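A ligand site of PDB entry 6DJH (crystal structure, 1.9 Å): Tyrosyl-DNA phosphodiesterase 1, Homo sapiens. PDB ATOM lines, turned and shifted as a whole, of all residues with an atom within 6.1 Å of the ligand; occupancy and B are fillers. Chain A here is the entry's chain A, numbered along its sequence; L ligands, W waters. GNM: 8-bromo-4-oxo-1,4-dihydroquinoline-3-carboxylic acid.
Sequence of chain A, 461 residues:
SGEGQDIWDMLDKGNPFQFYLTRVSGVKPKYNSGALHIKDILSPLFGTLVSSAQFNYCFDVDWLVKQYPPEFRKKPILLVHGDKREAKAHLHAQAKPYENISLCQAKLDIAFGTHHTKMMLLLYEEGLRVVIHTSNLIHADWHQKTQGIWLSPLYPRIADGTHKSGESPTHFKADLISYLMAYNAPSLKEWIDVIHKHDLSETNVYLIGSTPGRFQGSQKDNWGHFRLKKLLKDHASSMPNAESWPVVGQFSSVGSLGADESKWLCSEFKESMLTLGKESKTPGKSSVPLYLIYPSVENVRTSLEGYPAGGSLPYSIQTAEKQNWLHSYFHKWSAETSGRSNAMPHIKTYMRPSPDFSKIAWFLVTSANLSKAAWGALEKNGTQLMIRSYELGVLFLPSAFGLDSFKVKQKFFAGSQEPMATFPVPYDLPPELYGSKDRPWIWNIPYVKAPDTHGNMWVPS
The side-chain amino group (NZ) of Lys 118 lies within salt-bridge range of an oxygen (O01) of the ligand. An oxygen (O01) of the ligand lies within hydrogen-bond range of the side-chain amide nitrogen (ND2) of Asn 136 (2.9 Å). NE2 of His 346 lies within hydrogen-bond range of O15 of the ligand (2.8 Å).
NZ of Lys 118 is in hydrogen-bond range of O of His 116 (2.8 Å). The side-chain amino group (NZ) of Lys 348 is in hydrogen-bond range of the backbone carbonyl oxygen (O) of His 346 (2.6 Å). ND1 of His 346 lies within hydrogen-bond range of O of Thr 134 (2.8 Å). ND1 of His 116 lies within hydrogen-bond range of OE1 of Glu 391, 3.0 Å away. The backbone NH (N) of Cys 58 sits at hydrogen-bond distance from the side-chain amide oxygen (OD1) of Asn 136 (3.1 Å). OD1 of Asn 56 lies close to OD1 of Asn 136, 3.3 Å away. ND2 of Asn 136 lies within hydrogen-bond range of OD2 of Asp 141 (2.8 Å).
Merely in contact with the ligand: Tyr 57, His 116, Gly 311, Ser 312, Pro 314 and Trp 443. Hydrophobic or aromatic side chains that line the ligand: Tyr 57, His 116, Pro 314, His 346 and Trp 443. Of the 21 residues printed, 9 come within 4 Å of the ligand.
Water W1 bridges a ring nitrogen (NE2) of His 116 (2.8 Å) and a nitrogen (N06) of the ligand (2.9 Å). Water W3 lies within hydrogen-bond range of OD1 of Asp 141, OG of Ser 312, O15 of the ligand and ND2 of Asn 136.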
ATOM      1  N   ASN A  56       3.937   0.896   4.906  1.00  0.00           N
ATOM      2  CA  ASN A  56       4.556   2.125   4.445  1.00  0.00           C
ATOM      3  C   ASN A  56       4.171   3.269   5.365  1.00  0.00           C
ATOM      4  O   ASN A  56       3.526   3.087   6.396  1.00  0.00           O
ATOM      5  CB  ASN A  56       4.196   2.425   2.991  1.00  0.00           C
ATOM      6  CG  ASN A  56       5.367   3.058   2.254  1.00  0.00           C
ATOM      7  OD1 ASN A  56       5.741   4.179   2.563  1.00  0.00           O
ATOM      8  ND2 ASN A  56       5.976   2.313   1.328  1.00  0.00           N
ATOM      9  N   TYR A  57       4.623   4.466   4.994  1.00  0.00           N
ATOM     10  CA  TYR A  57       4.337   5.690   5.718  1.00  0.00           C
ATOM     11  C   TYR A  57       3.270   6.485   4.979  1.00  0.00           C
ATOM     12  O   TYR A  57       2.188   6.748   5.524  1.00  0.00           O
ATOM     13  CB  TYR A  57       5.631   6.497   5.883  1.00  0.00           C
ATOM     14  CG  TYR A  57       5.403   7.868   6.442  1.00  0.00           C
ATOM     15  CD1 TYR A  57       4.992   8.033   7.766  1.00  0.00           C
ATOM     16  CD2 TYR A  57       5.568   8.993   5.654  1.00  0.00           C
ATOM     17  CE1 TYR A  57       4.760   9.292   8.287  1.00  0.00           C
ATOM     18  CE2 TYR A  57       5.342  10.268   6.173  1.00  0.00           C
ATOM     19  CZ  TYR A  57       4.946  10.409   7.489  1.00  0.00           C
ATOM     20  OH  TYR A  57       4.722  11.665   7.998  1.00  0.00           O
ATOM     21  N   CYS A  58       3.530   6.846   3.732  1.00  0.00           N
ATOM     22  CA  CYS A  58       2.628   7.627   2.916  1.00  0.00           C
ATOM     23  C   CYS A  58       2.093   6.785   1.761  1.00  0.00           C
ATOM     24  O   CYS A  58       2.851   6.054   1.111  1.00  0.00           O
ATOM     25  CB  CYS A  58       3.331   8.869   2.366  1.00  0.00           C
ATOM     26  SG  CYS A  58       2.203  10.034   1.585  1.00  0.00           S
ATOM     27  N   HIS A 115       5.222   5.382  11.765  1.00  0.00           N
ATOM     28  CA  HIS A 115       5.408   4.076  11.122  1.00  0.00           C
ATOM     29  C   HIS A 115       6.155   4.295   9.812  1.00  0.00           C
ATOM     30  O   HIS A 115       5.552   4.574   8.774  1.00  0.00           O
ATOM     31  CB  HIS A 115       4.083   3.361  10.862  1.00  0.00           C
ATOM     32  CG  HIS A 115       4.251   1.985  10.290  1.00  0.00           C
ATOM     33  ND1 HIS A 115       4.215   1.738   8.930  1.00  0.00           N
ATOM     34  CD2 HIS A 115       4.487   0.790  10.881  1.00  0.00           C
ATOM     35  CE1 HIS A 115       4.411   0.451   8.722  1.00  0.00           C
ATOM     36  NE2 HIS A 115       4.578  -0.149   9.878  1.00  0.00           N
ATOM     37  N   HIS A 116       7.485   4.166   9.859  1.00  0.00           N
ATOM     38  CA  HIS A 116       8.332   4.446   8.706  1.00  0.00           C
ATOM     39  C   HIS A 116       8.718   3.216   7.893  1.00  0.00           C
ATOM     40  O   HIS A 116       9.238   3.377   6.782  1.00  0.00           O
ATOM     41  CB  HIS A 116       9.608   5.171   9.133  1.00  0.00           C
ATOM     42  CG  HIS A 116       9.394   6.631   9.425  1.00  0.00           C
ATOM     43  ND1 HIS A 116      10.158   7.326  10.341  1.00  0.00           N
ATOM     44  CD2 HIS A 116       8.489   7.507   8.933  1.00  0.00           C
ATOM     45  CE1 HIS A 116       9.747   8.581  10.374  1.00  0.00           C
ATOM     46  NE2 HIS A 116       8.724   8.716   9.553  1.00  0.00           N
ATOM     47  N   LYS A 118       9.122   0.335   5.370  1.00  0.00           N
ATOM     48  CA  LYS A 118       8.708   0.160   3.983  1.00  0.00           C
ATOM     49  C   LYS A 118       9.004  -1.270   3.552  1.00  0.00           C
ATOM     50  O   LYS A 118      10.164  -1.666   3.386  1.00  0.00           O
ATOM     51  CB  LYS A 118       9.400   1.208   3.114  1.00  0.00           C
ATOM     52  CG  LYS A 118       8.952   2.592   3.604  1.00  0.00           C
ATOM     53  CD  LYS A 118       9.425   3.721   2.780  1.00  0.00           C
ATOM     54  CE  LYS A 118       8.848   5.009   3.355  1.00  0.00           C
ATOM     55  NZ  LYS A 118       9.477   5.275   4.675  1.00  0.00           N
ATOM     56  N   THR A 134      12.812   1.595   0.533  1.00  0.00           N
ATOM     57  CA  THR A 134      12.872   2.910   1.159  1.00  0.00           C
ATOM     58  C   THR A 134      11.887   3.914   0.588  1.00  0.00           C
ATOM     59  O   THR A 134      11.874   5.060   1.038  1.00  0.00           O
ATOM     60  CB  THR A 134      14.302   3.503   1.049  1.00  0.00           C
ATOM     61  OG1 THR A 134      14.613   3.788  -0.326  1.00  0.00           O
ATOM     62  CG2 THR A 134      15.354   2.539   1.564  1.00  0.00           C
ATOM     63  N   SER A 135      11.021   3.524  -0.351  1.00  0.00           N
ATOM     64  CA  SER A 135      10.139   4.461  -1.024  1.00  0.00           C
ATOM     65  C   SER A 135       8.728   4.470  -0.433  1.00  0.00           C
ATOM     66  O   SER A 135       8.142   3.405  -0.186  1.00  0.00           O
ATOM     67  CB  SER A 135       9.998   4.145  -2.507  1.00  0.00           C
ATOM     68  OG  SER A 135      11.256   4.121  -3.129  1.00  0.00           O
ATOM     69  N   ASN A 136       8.163   5.670  -0.293  1.00  0.00           N
ATOM     70  CA  ASN A 136       6.732   5.783  -0.015  1.00  0.00           C
ATOM     71  C   ASN A 136       5.947   5.340  -1.246  1.00  0.00           C
ATOM     72  O   ASN A 136       6.475   5.288  -2.356  1.00  0.00           O
ATOM     73  CB  ASN A 136       6.345   7.211   0.354  1.00  0.00           C
ATOM     74  CG  ASN A 136       6.957   7.660   1.659  1.00  0.00           C
ATOM     75  OD1 ASN A 136       6.445   7.360   2.740  1.00  0.00           O
ATOM     76  ND2 ASN A 136       8.072   8.398   1.570  1.00  0.00           N
ATOM     77  N   ASP A 141       8.004   9.425  -5.166  1.00  0.00           N
ATOM     78  CA  ASP A 141       9.086   8.665  -4.561  1.00  0.00           C
ATOM     79  C   ASP A 141       9.724   7.668  -5.521  1.00  0.00           C
ATOM     80  O   ASP A 141      10.855   7.242  -5.270  1.00  0.00           O
ATOM     81  CB  ASP A 141       8.603   7.955  -3.297  1.00  0.00           C
ATOM     82  CG  ASP A 141       8.861   8.779  -2.035  1.00  0.00           C
ATOM     83  OD1 ASP A 141       8.644  10.015  -2.092  1.00  0.00           O
ATOM     84  OD2 ASP A 141       9.288   8.232  -0.999  1.00  0.00           O
ATOM     85  N   SER A 252      18.089  11.057   4.792  1.00  0.00           N
ATOM     86  CA  SER A 252      17.345  12.164   4.206  1.00  0.00           C
ATOM     87  C   SER A 252      16.687  13.069   5.243  1.00  0.00           C
ATOM     88  O   SER A 252      16.019  14.033   4.852  1.00  0.00           O
ATOM     89  CB  SER A 252      16.289  11.643   3.220  1.00  0.00           C
ATOM     90  OG  SER A 252      15.475  10.657   3.799  1.00  0.00           O
ATOM     91  N   GLY A 311      10.994  18.885  -0.395  1.00  0.00           N
ATOM     92  CA  GLY A 311       9.800  18.480   0.316  1.00  0.00           C
ATOM     93  C   GLY A 311       9.946  17.119   0.977  1.00  0.00           C
ATOM     94  O   GLY A 311       9.206  16.800   1.914  1.00  0.00           O
ATOM     95  N   SER A 312      10.902  16.310   0.515  1.00  0.00           N
ATOM     96  CA  SER A 312      11.150  14.979   1.059  1.00  0.00           C
ATOM     97  C   SER A 312      12.439  14.914   1.874  1.00  0.00           C
ATOM     98  O   SER A 312      12.958  13.816   2.124  1.00  0.00           O
ATOM     99  CB  SER A 312      11.191  13.940  -0.062  1.00  0.00           C
ATOM    100  OG  SER A 312       9.947  13.869  -0.724  1.00  0.00           O
ATOM    101  N   LEU A 313      12.971  16.063   2.265  1.00  0.00           N
ATOM    102  CA  LEU A 313      14.166  16.150   3.102  1.00  0.00           C
ATOM    103  C   LEU A 313      13.784  17.068   4.256  1.00  0.00           C
ATOM    104  O   LEU A 313      14.191  18.228   4.308  1.00  0.00           O
ATOM    105  CB  LEU A 313      15.360  16.673   2.309  1.00  0.00           C
ATOM    106  CG  LEU A 313      15.785  15.869   1.070  1.00  0.00           C
ATOM    107  CD1 LEU A 313      16.647  16.704   0.126  1.00  0.00           C
ATOM    108  CD2 LEU A 313      16.546  14.615   1.474  1.00  0.00           C
ATOM    109  N   PRO A 314      12.994  16.571   5.214  1.00  0.00           N
ATOM    110  CA  PRO A 314      12.286  17.451   6.162  1.00  0.00           C
ATOM    111  C   PRO A 314      13.116  17.847   7.386  1.00  0.00           C
ATOM    112  O   PRO A 314      12.740  17.589   8.529  1.00  0.00           O
ATOM    113  CB  PRO A 314      11.059  16.612   6.543  1.00  0.00           C
ATOM    114  CG  PRO A 314      11.549  15.204   6.479  1.00  0.00           C
ATOM    115  CD  PRO A 314      12.577  15.157   5.367  1.00  0.00           C
ATOM    116  N   HIS A 346      16.415   9.463  -1.118  1.00  0.00           N
ATOM    117  CA  HIS A 346      15.480   9.085  -0.067  1.00  0.00           C
ATOM    118  C   HIS A 346      15.842   7.728   0.519  1.00  0.00           C
ATOM    119  O   HIS A 346      15.232   7.310   1.515  1.00  0.00           O
ATOM    120  CB  HIS A 346      14.047   9.120  -0.617  1.00  0.00           C
ATOM    121  CG  HIS A 346      12.989   8.972   0.436  1.00  0.00           C
ATOM    122  ND1 HIS A 346      12.399   7.764   0.734  1.00  0.00           N
ATOM    123  CD2 HIS A 346      12.403   9.891   1.244  1.00  0.00           C
ATOM    124  CE1 HIS A 346      11.491   7.942   1.683  1.00  0.00           C
ATOM    125  NE2 HIS A 346      11.485   9.220   2.026  1.00  0.00           N
ATOM    126  N   LYS A 348      18.380   5.428   2.766  1.00  0.00           N
ATOM    127  CA  LYS A 348      19.219   5.658   3.941  1.00  0.00           C
ATOM    128  C   LYS A 348      20.169   4.482   4.035  1.00  0.00           C
ATOM    129  O   LYS A 348      19.731   3.334   3.913  1.00  0.00           O
ATOM    130  CB  LYS A 348      18.411   5.768   5.266  1.00  0.00           C
ATOM    131  CG  LYS A 348      17.419   6.930   5.281  1.00  0.00           C
ATOM    132  CD  LYS A 348      16.026   6.490   4.835  1.00  0.00           C
ATOM    133  CE  LYS A 348      15.044   7.636   4.952  1.00  0.00           C
ATOM    134  NZ  LYS A 348      14.098   7.631   3.818  1.00  0.00           N
ATOM    135  N   SER A 367      15.042   2.143   6.375  1.00  0.00           N
ATOM    136  CA  SER A 367      14.166   3.309   6.434  1.00  0.00           C
ATOM    137  C   SER A 367      14.599   4.287   7.520  1.00  0.00           C
ATOM    138  O   SER A 367      14.100   5.413   7.541  1.00  0.00           O
ATOM    139  CB  SER A 367      12.720   2.854   6.693  1.00  0.00           C
ATOM    140  OG  SER A 367      12.616   2.194   7.964  1.00  0.00           O
ATOM    141  N   ASN A 369      16.251   7.122   9.501  1.00  0.00           N
ATOM    142  CA  ASN A 369      17.040   8.337   9.374  1.00  0.00           C
ATOM    143  C   ASN A 369      17.936   8.513  10.598  1.00  0.00           C
ATOM    144  O   ASN A 369      17.979   7.658  11.499  1.00  0.00           O
ATOM    145  CB  ASN A 369      16.125   9.555   9.177  1.00  0.00           C
ATOM    146  CG  ASN A 369      15.688   9.730   7.745  1.00  0.00           C
ATOM    147  OD1 ASN A 369      16.510   9.709   6.838  1.00  0.00           O
ATOM    148  ND2 ASN A 369      14.380   9.859   7.527  1.00  0.00           N
ATOM    149  N   GLU A 391      10.771   0.966  12.124  1.00  0.00           N
ATOM    150  CA  GLU A 391      11.737   1.072  11.028  1.00  0.00           C
ATOM    151  C   GLU A 391      12.186  -0.329  10.667  1.00  0.00           C
ATOM    152  O   GLU A 391      12.110  -1.249  11.497  1.00  0.00           O
ATOM    153  CB  GLU A 391      12.994   1.886  11.387  1.00  0.00           C
ATOM    154  CG  GLU A 391      12.712   3.179  12.146  1.00  0.00           C
ATOM    155  CD  GLU A 391      12.436   4.347  11.208  1.00  0.00           C
ATOM    156  OE1 GLU A 391      12.071   5.450  11.693  1.00  0.00           O
ATOM    157  OE2 GLU A 391      12.570   4.159   9.982  1.00  0.00           O
ATOM    158  N   TRP A 443      14.207  22.583   5.142  1.00  0.00           N
ATOM    159  CA  TRP A 443      13.076  22.646   4.214  1.00  0.00           C
ATOM    160  C   TRP A 443      12.116  23.799   4.477  1.00  0.00           C
ATOM    161  O   TRP A 443      11.387  24.180   3.569  1.00  0.00           O
ATOM    162  CB  TRP A 443      12.280  21.332   4.189  1.00  0.00           C
ATOM    163  CG  TRP A 443      11.422  21.052   5.371  1.00  0.00           C
ATOM    164  CD1 TRP A 443      11.612  21.473   6.658  1.00  0.00           C
ATOM    165  CD2 TRP A 443      10.246  20.239   5.387  1.00  0.00           C
ATOM    166  NE1 TRP A 443      10.612  20.992   7.466  1.00  0.00           N
ATOM    167  CE2 TRP A 443       9.756  20.224   6.713  1.00  0.00           C
ATOM    168  CE3 TRP A 443       9.546  19.529   4.396  1.00  0.00           C
ATOM    169  CZ2 TRP A 443       8.604  19.530   7.082  1.00  0.00           C
ATOM    170  CZ3 TRP A 443       8.391  18.848   4.768  1.00  0.00           C
ATOM    171  CH2 TRP A 443       7.934  18.840   6.097  1.00  0.00           C
HETATM  172  C10 GNM L   1       8.153  14.996   5.346  1.00  0.00           C
HETATM  173  C13 GNM L   1       8.842  12.349   4.723  1.00  0.00           C
HETATM  174  C02 GNM L   1       9.409   8.598   5.241  1.00  0.00           C
HETATM  175  C04 GNM L   1       9.068  10.073   5.449  1.00  0.00           C
HETATM  176  C05 GNM L   1       8.641  10.491   6.702  1.00  0.00           C
HETATM  177  C07 GNM L   1       8.427  12.678   5.994  1.00  0.00           C
HETATM  178  C08 GNM L   1       8.072  14.006   6.310  1.00  0.00           C
HETATM  179  C11 GNM L   1       8.576  14.681   4.049  1.00  0.00           C
HETATM  180  C12 GNM L   1       8.919  13.364   3.739  1.00  0.00           C
HETATM  181  C14 GNM L   1       9.171  11.020   4.425  1.00  0.00           C
HETATM  182  N06 GNM L   1       8.330  11.750   6.963  1.00  0.00           N
HETATM  183  O01 GNM L   1       9.433   8.104   4.097  1.00  0.00           O
HETATM  184  O03 GNM L   1       9.662   7.884   6.243  1.00  0.00           O
HETATM  185  O15 GNM L   1       9.531  10.728   3.327  1.00  0.00           O
HETATM  186 BR9  GNM L   1       7.504  14.400   8.120  1.00  0.00          BR
HETATM  187  O   HOH W   1       7.945  11.395   9.800  1.00  0.00           O
HETATM  188  O   HOH W   2       5.998  12.448   2.278  1.00  0.00           O
HETATM  189  O   HOH W   3       8.777  11.409   0.256  1.00  0.00           O
